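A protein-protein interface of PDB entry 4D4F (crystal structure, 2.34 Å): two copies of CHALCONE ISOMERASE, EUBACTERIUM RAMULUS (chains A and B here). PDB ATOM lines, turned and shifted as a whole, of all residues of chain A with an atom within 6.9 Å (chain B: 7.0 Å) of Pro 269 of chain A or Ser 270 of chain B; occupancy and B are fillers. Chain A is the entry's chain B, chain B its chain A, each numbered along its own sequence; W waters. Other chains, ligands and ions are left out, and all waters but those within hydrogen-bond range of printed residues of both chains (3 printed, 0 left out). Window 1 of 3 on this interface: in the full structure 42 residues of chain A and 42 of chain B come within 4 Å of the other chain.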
ATOM      1  N   PHE A  51      -9.585  12.595 -29.767  1.00  0.00           N
ATOM      2  CA  PHE A  51      -9.449  11.460 -28.872  1.00  0.00           C
ATOM      3  C   PHE A  51     -10.389  10.311 -29.307  1.00  0.00           C
ATOM      4  O   PHE A  51     -11.583  10.523 -29.604  1.00  0.00           O
ATOM      5  CB  PHE A  51      -9.835  11.846 -27.440  1.00  0.00           C
ATOM      6  CG  PHE A  51      -9.134  13.051 -26.882  1.00  0.00           C
ATOM      7  CD1 PHE A  51      -7.836  13.374 -27.228  1.00  0.00           C
ATOM      8  CD2 PHE A  51      -9.766  13.828 -25.932  1.00  0.00           C
ATOM      9  CE1 PHE A  51      -7.193  14.496 -26.661  1.00  0.00           C
ATOM     10  CE2 PHE A  51      -9.140  14.925 -25.349  1.00  0.00           C
ATOM     11  CZ  PHE A  51      -7.850  15.265 -25.718  1.00  0.00           C
ATOM     12  N   PRO A  53     -11.714   7.152 -27.450  1.00  0.00           N
ATOM     13  CA  PRO A  53     -11.849   6.352 -26.234  1.00  0.00           C
ATOM     14  C   PRO A  53     -11.772   4.855 -26.532  1.00  0.00           C
ATOM     15  O   PRO A  53     -12.363   4.375 -27.504  1.00  0.00           O
ATOM     16  CB  PRO A  53     -13.271   6.676 -25.745  1.00  0.00           C
ATOM     17  CG  PRO A  53     -13.609   7.984 -26.382  1.00  0.00           C
ATOM     18  CD  PRO A  53     -12.871   8.021 -27.687  1.00  0.00           C
ATOM     19  N   TYR A 267     -15.966   6.100 -35.055  1.00  0.00           N
ATOM     20  CA  TYR A 267     -16.350   7.488 -34.873  1.00  0.00           C
ATOM     21  C   TYR A 267     -16.002   7.942 -33.467  1.00  0.00           C
ATOM     22  O   TYR A 267     -16.181   7.180 -32.499  1.00  0.00           O
ATOM     23  CB  TYR A 267     -17.862   7.642 -35.105  1.00  0.00           C
ATOM     24  CG  TYR A 267     -18.418   8.971 -34.670  1.00  0.00           C
ATOM     25  CD1 TYR A 267     -18.326  10.082 -35.489  1.00  0.00           C
ATOM     26  CD2 TYR A 267     -18.993   9.136 -33.424  1.00  0.00           C
ATOM     27  CE1 TYR A 267     -18.802  11.331 -35.073  1.00  0.00           C
ATOM     28  CE2 TYR A 267     -19.506  10.367 -33.010  1.00  0.00           C
ATOM     29  CZ  TYR A 267     -19.418  11.463 -33.840  1.00  0.00           C
ATOM     30  OH  TYR A 267     -19.899  12.690 -33.438  1.00  0.00           O
ATOM     31  N   THR A 268     -15.540   9.189 -33.354  1.00  0.00           N
ATOM     32  CA  THR A 268     -15.455   9.847 -32.050  1.00  0.00           C
ATOM     33  C   THR A 268     -16.196  11.189 -32.029  1.00  0.00           C
ATOM     34  O   THR A 268     -16.082  11.977 -32.965  1.00  0.00           O
ATOM     35  CB  THR A 268     -13.997  10.049 -31.577  1.00  0.00           C
ATOM     36  OG1 THR A 268     -14.022  10.615 -30.266  1.00  0.00           O
ATOM     37  CG2 THR A 268     -13.172  10.961 -32.549  1.00  0.00           C
ATOM     38  N   PRO A 269     -16.947  11.454 -30.958  1.00  0.00           N
ATOM     39  CA  PRO A 269     -17.488  12.796 -30.783  1.00  0.00           C
ATOM     40  C   PRO A 269     -16.413  13.784 -30.372  1.00  0.00           C
ATOM     41  O   PRO A 269     -16.655  14.973 -30.411  1.00  0.00           O
ATOM     42  CB  PRO A 269     -18.504  12.640 -29.670  1.00  0.00           C
ATOM     43  CG  PRO A 269     -18.104  11.418 -28.933  1.00  0.00           C
ATOM     44  CD  PRO A 269     -17.266  10.566 -29.834  1.00  0.00           C
ATOM     45  N   SER A 270     -15.229  13.301 -30.003  1.00  0.00           N
ATOM     46  CA  SER A 270     -14.180  14.200 -29.546  1.00  0.00           C
ATOM     47  C   SER A 270     -13.221  14.571 -30.670  1.00  0.00           C
ATOM     48  O   SER A 270     -12.039  14.192 -30.686  1.00  0.00           O
ATOM     49  CB  SER A 270     -13.450  13.594 -28.353  1.00  0.00           C
ATOM     50  OG  SER A 270     -14.336  13.476 -27.262  1.00  0.00           O
ATOM     51  N   ASN A 271     -13.766  15.288 -31.633  1.00  0.00           N
ATOM     52  CA  ASN A 271     -12.969  15.875 -32.697  1.00  0.00           C
ATOM     53  C   ASN A 271     -12.731  17.324 -32.306  1.00  0.00           C
ATOM     54  O   ASN A 271     -13.512  18.227 -32.652  1.00  0.00           O
ATOM     55  CB  ASN A 271     -13.678  15.800 -34.052  1.00  0.00           C
ATOM     56  CG  ASN A 271     -12.764  16.234 -35.196  1.00  0.00           C
ATOM     57  OD1 ASN A 271     -11.538  16.108 -35.095  1.00  0.00           O
ATOM     58  ND2 ASN A 271     -13.349  16.750 -36.279  1.00  0.00           N
ATOM     59  N   ASN A 272     -11.653  17.513 -31.566  1.00  0.00           N
ATOM     60  CA  ASN A 272     -11.554  18.631 -30.647  1.00  0.00           C
ATOM     61  C   ASN A 272     -11.478  19.999 -31.277  1.00  0.00           C
ATOM     62  O   ASN A 272     -11.992  20.951 -30.697  1.00  0.00           O
ATOM     63  CB  ASN A 272     -10.381  18.438 -29.718  1.00  0.00           C
ATOM     64  CG  ASN A 272     -10.529  17.203 -28.868  1.00  0.00           C
ATOM     65  OD1 ASN A 272     -11.625  16.851 -28.456  1.00  0.00           O
ATOM     66  ND2 ASN A 272      -9.413  16.548 -28.579  1.00  0.00           N
ATOM     67  N   ASN A 275     -15.346  20.494 -32.420  1.00  0.00           N
ATOM     68  CA  ASN A 275     -16.480  20.165 -31.557  1.00  0.00           C
ATOM     69  C   ASN A 275     -16.417  20.647 -30.100  1.00  0.00           C
ATOM     70  O   ASN A 275     -17.440  20.614 -29.427  1.00  0.00           O
ATOM     71  CB  ASN A 275     -16.688  18.607 -31.505  1.00  0.00           C
ATOM     72  CG  ASN A 275     -16.934  17.972 -32.892  1.00  0.00           C
ATOM     73  OD1 ASN A 275     -17.111  18.661 -33.915  1.00  0.00           O
ATOM     74  ND2 ASN A 275     -16.937  16.651 -32.926  1.00  0.00           N
ATOM     75  N   TYR A 276     -15.267  21.070 -29.593  1.00  0.00           N
ATOM     76  CA  TYR A 276     -15.160  21.455 -28.183  1.00  0.00           C
ATOM     77  C   TYR A 276     -15.786  22.797 -27.859  1.00  0.00           C
ATOM     78  O   TYR A 276     -15.482  23.785 -28.518  1.00  0.00           O
ATOM     79  CB  TYR A 276     -13.686  21.528 -27.771  1.00  0.00           C
ATOM     80  CG  TYR A 276     -13.440  21.645 -26.296  1.00  0.00           C
ATOM     81  CD1 TYR A 276     -13.760  20.587 -25.433  1.00  0.00           C
ATOM     82  CD2 TYR A 276     -12.888  22.785 -25.762  1.00  0.00           C
ATOM     83  CE1 TYR A 276     -13.533  20.677 -24.067  1.00  0.00           C
ATOM     84  CE2 TYR A 276     -12.659  22.889 -24.394  1.00  0.00           C
ATOM     85  CZ  TYR A 276     -12.974  21.826 -23.542  1.00  0.00           C
ATOM     86  OH  TYR A 276     -12.715  21.906 -22.180  1.00  0.00           O
ATOM     87  N   GLN B  27     -23.318   1.183 -30.733  1.00  0.00           N
ATOM     88  CA  GLN B  27     -22.706   2.489 -30.705  1.00  0.00           C
ATOM     89  C   GLN B  27     -22.789   3.168 -32.076  1.00  0.00           C
ATOM     90  O   GLN B  27     -23.057   4.355 -32.174  1.00  0.00           O
ATOM     91  CB  GLN B  27     -21.260   2.366 -30.221  1.00  0.00           C
ATOM     92  CG  GLN B  27     -20.575   3.682 -29.940  1.00  0.00           C
ATOM     93  CD  GLN B  27     -19.404   3.477 -29.003  1.00  0.00           C
ATOM     94  OE1 GLN B  27     -19.560   2.872 -27.962  1.00  0.00           O
ATOM     95  NE2 GLN B  27     -18.234   3.951 -29.383  1.00  0.00           N
ATOM     96  N   TYR B  31     -24.831   6.668 -32.917  1.00  0.00           N
ATOM     97  CA  TYR B  31     -24.136   7.879 -33.355  1.00  0.00           C
ATOM     98  C   TYR B  31     -24.324   8.201 -34.849  1.00  0.00           C
ATOM     99  O   TYR B  31     -24.301   9.361 -35.237  1.00  0.00           O
ATOM    100  CB  TYR B  31     -22.634   7.803 -32.968  1.00  0.00           C
ATOM    101  CG  TYR B  31     -22.425   8.104 -31.516  1.00  0.00           C
ATOM    102  CD1 TYR B  31     -22.282   9.421 -31.086  1.00  0.00           C
ATOM    103  CD2 TYR B  31     -22.460   7.102 -30.563  1.00  0.00           C
ATOM    104  CE1 TYR B  31     -22.152   9.737 -29.758  1.00  0.00           C
ATOM    105  CE2 TYR B  31     -22.329   7.407 -29.216  1.00  0.00           C
ATOM    106  CZ  TYR B  31     -22.151   8.742 -28.840  1.00  0.00           C
ATOM    107  OH  TYR B  31     -22.047   9.092 -27.537  1.00  0.00           O
ATOM    108  N   ILE B  35     -28.954   9.742 -33.870  1.00  0.00           N
ATOM    109  CA  ILE B  35     -28.788  11.181 -33.667  1.00  0.00           C
ATOM    110  C   ILE B  35     -29.471  11.991 -34.784  1.00  0.00           C
ATOM    111  O   ILE B  35     -30.304  12.879 -34.521  1.00  0.00           O
ATOM    112  CB  ILE B  35     -27.301  11.586 -33.560  1.00  0.00           C
ATOM    113  CG1 ILE B  35     -26.731  11.164 -32.231  1.00  0.00           C
ATOM    114  CG2 ILE B  35     -27.115  13.102 -33.731  1.00  0.00           C
ATOM    115  CD1 ILE B  35     -25.235  11.435 -32.085  1.00  0.00           C
ATOM    116  N   LYS B  48     -32.089  20.460 -25.425  1.00  0.00           N
ATOM    117  CA  LYS B  48     -30.800  19.785 -25.201  1.00  0.00           C
ATOM    118  C   LYS B  48     -30.988  18.291 -25.384  1.00  0.00           C
ATOM    119  O   LYS B  48     -31.982  17.718 -24.915  1.00  0.00           O
ATOM    120  CB  LYS B  48     -30.304  20.097 -23.777  1.00  0.00           C
ATOM    121  CG  LYS B  48     -28.880  19.702 -23.472  1.00  0.00           C
ATOM    122  CD  LYS B  48     -28.489  20.021 -22.010  1.00  0.00           C
ATOM    123  CE  LYS B  48     -27.252  19.227 -21.575  1.00  0.00           C
ATOM    124  NZ  LYS B  48     -26.068  19.670 -22.340  1.00  0.00           N
ATOM    125  N   TYR B  49     -30.013  17.669 -26.021  1.00  0.00           N
ATOM    126  CA  TYR B  49     -30.089  16.248 -26.320  1.00  0.00           C
ATOM    127  C   TYR B  49     -28.690  15.712 -26.234  1.00  0.00           C
ATOM    128  O   TYR B  49     -27.858  16.102 -27.044  1.00  0.00           O
ATOM    129  CB  TYR B  49     -30.646  16.090 -27.746  1.00  0.00           C
ATOM    130  CG  TYR B  49     -30.595  14.716 -28.364  1.00  0.00           C
ATOM    131  CD1 TYR B  49     -30.959  13.599 -27.658  1.00  0.00           C
ATOM    132  CD2 TYR B  49     -30.218  14.547 -29.704  1.00  0.00           C
ATOM    133  CE1 TYR B  49     -30.935  12.325 -28.249  1.00  0.00           C
ATOM    134  CE2 TYR B  49     -30.211  13.286 -30.296  1.00  0.00           C
ATOM    135  CZ  TYR B  49     -30.569  12.181 -29.559  1.00  0.00           C
ATOM    136  OH  TYR B  49     -30.570  10.943 -30.121  1.00  0.00           O
ATOM    137  N   ALA B  50     -28.429  14.827 -25.279  1.00  0.00           N
ATOM    138  CA  ALA B  50     -27.041  14.444 -24.947  1.00  0.00           C
ATOM    139  C   ALA B  50     -26.939  13.016 -24.515  1.00  0.00           C
ATOM    140  O   ALA B  50     -27.882  12.472 -23.973  1.00  0.00           O
ATOM    141  CB  ALA B  50     -26.500  15.341 -23.826  1.00  0.00           C
ATOM    142  N   PHE B  51     -25.786  12.412 -24.756  1.00  0.00           N
ATOM    143  CA  PHE B  51     -25.522  11.090 -24.276  1.00  0.00           C
ATOM    144  C   PHE B  51     -24.387  11.142 -23.259  1.00  0.00           C
ATOM    145  O   PHE B  51     -23.394  11.805 -23.504  1.00  0.00           O
ATOM    146  CB  PHE B  51     -25.067  10.190 -25.407  1.00  0.00           C
ATOM    147  CG  PHE B  51     -25.984  10.144 -26.595  1.00  0.00           C
ATOM    148  CD1 PHE B  51     -27.365  10.222 -26.460  1.00  0.00           C
ATOM    149  CD2 PHE B  51     -25.461   9.951 -27.860  1.00  0.00           C
ATOM    150  CE1 PHE B  51     -28.183  10.116 -27.574  1.00  0.00           C
ATOM    151  CE2 PHE B  51     -26.289   9.860 -28.966  1.00  0.00           C
ATOM    152  CZ  PHE B  51     -27.635   9.951 -28.819  1.00  0.00           C
ATOM    153  N   TYR B  52     -24.522  10.423 -22.146  1.00  0.00           N
ATOM    154  CA  TYR B  52     -23.462  10.327 -21.119  1.00  0.00           C
ATOM    155  C   TYR B  52     -23.002   8.850 -21.093  1.00  0.00           C
ATOM    156  O   TYR B  52     -23.668   7.993 -20.524  1.00  0.00           O
ATOM    157  CB  TYR B  52     -23.984  10.817 -19.741  1.00  0.00           C
ATOM    158  CG  TYR B  52     -24.500  12.265 -19.767  1.00  0.00           C
ATOM    159  CD1 TYR B  52     -25.804  12.550 -20.174  1.00  0.00           C
ATOM    160  CD2 TYR B  52     -23.665  13.353 -19.458  1.00  0.00           C
ATOM    161  CE1 TYR B  52     -26.255  13.860 -20.254  1.00  0.00           C
ATOM    162  CE2 TYR B  52     -24.126  14.659 -19.539  1.00  0.00           C
ATOM    163  CZ  TYR B  52     -25.422  14.910 -19.929  1.00  0.00           C
ATOM    164  OH  TYR B  52     -25.895  16.221 -20.004  1.00  0.00           O
ATOM    165  N   PRO B  53     -21.889   8.545 -21.764  1.00  0.00           N
ATOM    166  CA  PRO B  53     -21.424   7.160 -21.732  1.00  0.00           C
ATOM    167  C   PRO B  53     -21.104   6.736 -20.323  1.00  0.00           C
ATOM    168  O   PRO B  53     -20.618   7.541 -19.533  1.00  0.00           O
ATOM    169  CB  PRO B  53     -20.142   7.166 -22.578  1.00  0.00           C
ATOM    170  CG  PRO B  53     -19.840   8.594 -22.860  1.00  0.00           C
ATOM    171  CD  PRO B  53     -21.102   9.385 -22.677  1.00  0.00           C
ATOM    172  N   GLN B  70     -24.961   3.818 -22.145  1.00  0.00           N
ATOM    173  CA  GLN B  70     -25.065   5.244 -21.808  1.00  0.00           C
ATOM    174  C   GLN B  70     -26.340   5.586 -21.089  1.00  0.00           C
ATOM    175  O   GLN B  70     -27.243   4.775 -20.984  1.00  0.00           O
ATOM    176  CB  GLN B  70     -24.987   6.095 -23.084  1.00  0.00           C
ATOM    177  CG  GLN B  70     -26.167   5.898 -24.029  1.00  0.00           C
ATOM    178  CD  GLN B  70     -25.917   6.453 -25.415  1.00  0.00           C
ATOM    179  OE1 GLN B  70     -24.867   6.229 -26.017  1.00  0.00           O
ATOM    180  NE2 GLN B  70     -26.907   7.162 -25.945  1.00  0.00           N
ATOM    181  N   TYR B 267     -18.867  15.587 -17.414  1.00  0.00           N
ATOM    182  CA  TYR B 267     -18.874  16.140 -18.766  1.00  0.00           C
ATOM    183  C   TYR B 267     -19.067  15.057 -19.799  1.00  0.00           C
ATOM    184  O   TYR B 267     -18.543  13.974 -19.675  1.00  0.00           O
ATOM    185  CB  TYR B 267     -17.516  16.789 -19.058  1.00  0.00           C
ATOM    186  CG  TYR B 267     -17.274  17.171 -20.515  1.00  0.00           C
ATOM    187  CD1 TYR B 267     -17.786  18.358 -21.046  1.00  0.00           C
ATOM    188  CD2 TYR B 267     -16.495  16.377 -21.343  1.00  0.00           C
ATOM    189  CE1 TYR B 267     -17.551  18.725 -22.373  1.00  0.00           C
ATOM    190  CE2 TYR B 267     -16.257  16.736 -22.662  1.00  0.00           C
ATOM    191  CZ  TYR B 267     -16.807  17.906 -23.176  1.00  0.00           C
ATOM    192  OH  TYR B 267     -16.522  18.279 -24.462  1.00  0.00           O
ATOM    193  N   THR B 268     -19.766  15.394 -20.858  1.00  0.00           N
ATOM    194  CA  THR B 268     -19.791  14.553 -22.029  1.00  0.00           C
ATOM    195  C   THR B 268     -19.498  15.371 -23.284  1.00  0.00           C
ATOM    196  O   THR B 268     -19.989  16.466 -23.428  1.00  0.00           O
ATOM    197  CB  THR B 268     -21.155  13.858 -22.233  1.00  0.00           C
ATOM    198  OG1 THR B 268     -21.060  13.017 -23.373  1.00  0.00           O
ATOM    199  CG2 THR B 268     -22.283  14.860 -22.517  1.00  0.00           C
ATOM    200  N   PRO B 269     -18.733  14.809 -24.204  1.00  0.00           N
ATOM    201  CA  PRO B 269     -18.586  15.452 -25.482  1.00  0.00           C
ATOM    202  C   PRO B 269     -19.808  15.291 -26.397  1.00  0.00           C
ATOM    203  O   PRO B 269     -19.905  16.005 -27.410  1.00  0.00           O
ATOM    204  CB  PRO B 269     -17.377  14.745 -26.101  1.00  0.00           C
ATOM    205  CG  PRO B 269     -17.362  13.408 -25.452  1.00  0.00           C
ATOM    206  CD  PRO B 269     -17.876  13.624 -24.060  1.00  0.00           C
ATOM    207  N   SER B 270     -20.735  14.384 -26.057  1.00  0.00           N
ATOM    208  CA  SER B 270     -21.904  14.111 -26.932  1.00  0.00           C
ATOM    209  C   SER B 270     -23.086  15.003 -26.523  1.00  0.00           C
ATOM    210  O   SER B 270     -24.137  14.517 -26.068  1.00  0.00           O
ATOM    211  CB  SER B 270     -22.277  12.637 -26.891  1.00  0.00           C
ATOM    212  OG  SER B 270     -21.171  11.894 -27.358  1.00  0.00           O
ATOM    213  N   ASN B 271     -22.866  16.311 -26.645  1.00  0.00           N
ATOM    214  CA  ASN B 271     -23.944  17.281 -26.566  1.00  0.00           C
ATOM    215  C   ASN B 271     -24.461  17.532 -27.951  1.00  0.00           C
ATOM    216  O   ASN B 271     -23.985  18.424 -28.682  1.00  0.00           O
ATOM    217  CB  ASN B 271     -23.496  18.585 -25.947  1.00  0.00           C
ATOM    218  CG  ASN B 271     -24.676  19.407 -25.487  1.00  0.00           C
ATOM    219  OD1 ASN B 271     -25.734  18.871 -25.162  1.00  0.00           O
ATOM    220  ND2 ASN B 271     -24.514  20.705 -25.460  1.00  0.00           N
ATOM    221  N   ASN B 272     -25.441  16.743 -28.312  1.00  0.00           N
ATOM    222  CA  ASN B 272     -25.721  16.508 -29.733  1.00  0.00           C
ATOM    223  C   ASN B 272     -26.260  17.669 -30.527  1.00  0.00           C
ATOM    224  O   ASN B 272     -25.938  17.776 -31.700  1.00  0.00           O
ATOM    225  CB  ASN B 272     -26.609  15.290 -29.914  1.00  0.00           C
ATOM    226  CG  ASN B 272     -26.013  14.049 -29.258  1.00  0.00           C
ATOM    227  OD1 ASN B 272     -24.812  13.827 -29.314  1.00  0.00           O
ATOM    228  ND2 ASN B 272     -26.858  13.255 -28.587  1.00  0.00           N
ATOM    229  N   LEU B 273     -27.069  18.532 -29.916  1.00  0.00           N
ATOM    230  CA  LEU B 273     -27.576  19.684 -30.656  1.00  0.00           C
ATOM    231  C   LEU B 273     -26.466  20.699 -30.948  1.00  0.00           C
ATOM    232  O   LEU B 273     -26.527  21.380 -31.931  1.00  0.00           O
ATOM    233  CB  LEU B 273     -28.765  20.340 -29.971  1.00  0.00           C
ATOM    234  CG  LEU B 273     -30.063  19.515 -29.895  1.00  0.00           C
ATOM    235  CD1 LEU B 273     -31.119  20.308 -29.137  1.00  0.00           C
ATOM    236  CD2 LEU B 273     -30.594  19.196 -31.264  1.00  0.00           C
ATOM    237  N   ASN B 275     -22.861  19.811 -30.922  1.00  0.00           N
ATOM    238  CA  ASN B 275     -21.562  19.223 -31.243  1.00  0.00           C
ATOM    239  C   ASN B 275     -21.531  18.250 -32.422  1.00  0.00           C
ATOM    240  O   ASN B 275     -20.451  17.866 -32.857  1.00  0.00           O
ATOM    241  CB  ASN B 275     -20.953  18.532 -29.998  1.00  0.00           C
ATOM    242  CG  ASN B 275     -20.729  19.506 -28.808  1.00  0.00           C
ATOM    243  OD1 ASN B 275     -21.019  20.698 -28.885  1.00  0.00           O
ATOM    244  ND2 ASN B 275     -20.228  18.984 -27.702  1.00  0.00           N
ATOM    245  N   TYR B 276     -22.673  17.876 -32.983  1.00  0.00           N
ATOM    246  CA  TYR B 276     -22.671  16.815 -33.987  1.00  0.00           C
ATOM    247  C   TYR B 276     -22.408  17.353 -35.380  1.00  0.00           C
ATOM    248  O   TYR B 276     -23.082  18.275 -35.816  1.00  0.00           O
ATOM    249  CB  TYR B 276     -24.007  16.078 -33.974  1.00  0.00           C
ATOM    250  CG  TYR B 276     -24.055  14.834 -34.826  1.00  0.00           C
ATOM    251  CD1 TYR B 276     -23.335  13.683 -34.453  1.00  0.00           C
ATOM    252  CD2 TYR B 276     -24.836  14.784 -35.983  1.00  0.00           C
ATOM    253  CE1 TYR B 276     -23.417  12.524 -35.205  1.00  0.00           C
ATOM    254  CE2 TYR B 276     -24.880  13.636 -36.766  1.00  0.00           C
ATOM    255  CZ  TYR B 276     -24.167  12.508 -36.368  1.00  0.00           C
ATOM    256  OH  TYR B 276     -24.208  11.333 -37.116  1.00  0.00           O
HETATM  257  O   HOH W   1     -18.279   5.803 -31.734  1.00  0.00           O
HETATM  258  O   HOH W   2     -14.364  16.393 -26.460  1.00  0.00           O
HETATM  259  O   HOH W   3     -15.816   4.329 -27.811  1.00  0.00           O
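Among the printed residues, pairs that only touch across the chains: Tyr 267 of chain A with Tyr 31 of chain B (3.5 Å), Tyr 267 of chain A with Tyr 276 of chain B (3.7 Å), Pro 269 of chain A with Ser 270 of chain B (3.5 Å), Ser 270 of chain A with Pro 269 of chain B (3.5 Å), Asn 275 of chain A with Asn 275 of chain B (3.5 Å) and Tyr 276 of chain A with Tyr 267 of chain B (3.7 Å).
Tyr 267 of chain A touches Tyr 276 of chain B, and with the chains exchanged Tyr 276 of chain A touches Tyr 267 of chain B.
Pro 269 of chain A touches Ser 270 of chain B, and with the chains exchanged Ser 270 of chain A touches Pro 269 of chain B.
Asn 275 of chain A touches its own counterpart, Asn 275 of chain B.
10 positions are printed for both chains.
Of the 6 pairs that touch across the chains among the printed residues, 5 have their exchanged pair printed and touching as well.
Of chain B, only Ser 270 (3.5 Å) comes within 4 Å of Pro 269 of chain A.
Ser 270 of chain B touches just one residue of chain A: Pro 269.
Of the printed residues of chain B, Tyr 267 of chain A touches Tyr 31 and Tyr 276.
Of the printed residues of chain A, Asn 275 of chain B touches Asn 275.
Of the printed residues of chain A, Tyr 31 of chain B touches Tyr 267.
Phe 51 of chain B touches none of the printed residues of chain A.
Water W1 lies within hydrogen-bond range of O of Tyr 267 of chain A (2.6 Å) and NE2 of Gln 27 of chain B (3.0 Å).
Water W3 bridges the side-chain amide nitrogen of Gln 27 of chain B (2.9 Å) and the backbone carbonyl oxygen of Pro 53 of chain A (3.5 Å).
Water W2 lies within hydrogen-bond range of OG of Ser 270 of chain A (3.0 Å), OD1 of Asn 272 of chain A (3.4 Å) and OH of Tyr 267 of chain B (3.5 Å).
Hydrophobic or aromatic side chains of chain A within 4 Å of the printed part of chain B: Tyr 267, Pro 269 and Tyr 276.
Of the 19 printed residues of chain B, 6 touch a printed residue of chain A.
Hydrophobic or aromatic side chains of chain B within 4 Å of the printed part of chain A: Tyr 31, Tyr 267, Pro 269 and Tyr 276.
The side-chain hydroxyl (OH) of Tyr 276 of chain B lies within hydrogen-bond range of the backbone carbonyl oxygen (O) of Tyr 31 of chain B, 2.7 Å away.
The side-chain hydroxyl (OG1) of Thr 268 of chain B is in hydrogen-bond range of the backbone NH (N) of Ser 270 of chain B.
The backbone NH of Phe 51 of chain A lies within hydrogen-bond range of the backbone carbonyl oxygen of Ser 270 of chain A (3.1 Å).
The backbone NH (N) of Ser 270 of chain A is in hydrogen-bond range of the side-chain hydroxyl (OG1) of Thr 268 of chain A (3.0 Å).
The side-chain amide nitrogen (ND2) of Asn 275 of chain A sits at hydrogen-bond distance from the backbone carbonyl oxygen (O) of Pro 269 of chain A (3.0 Å).
The backbone carbonyl oxygen (O) of Ser 270 of chain A sits close to the side-chain amide oxygen (OD1) of Asn 272 of chain A (3.5 Å).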
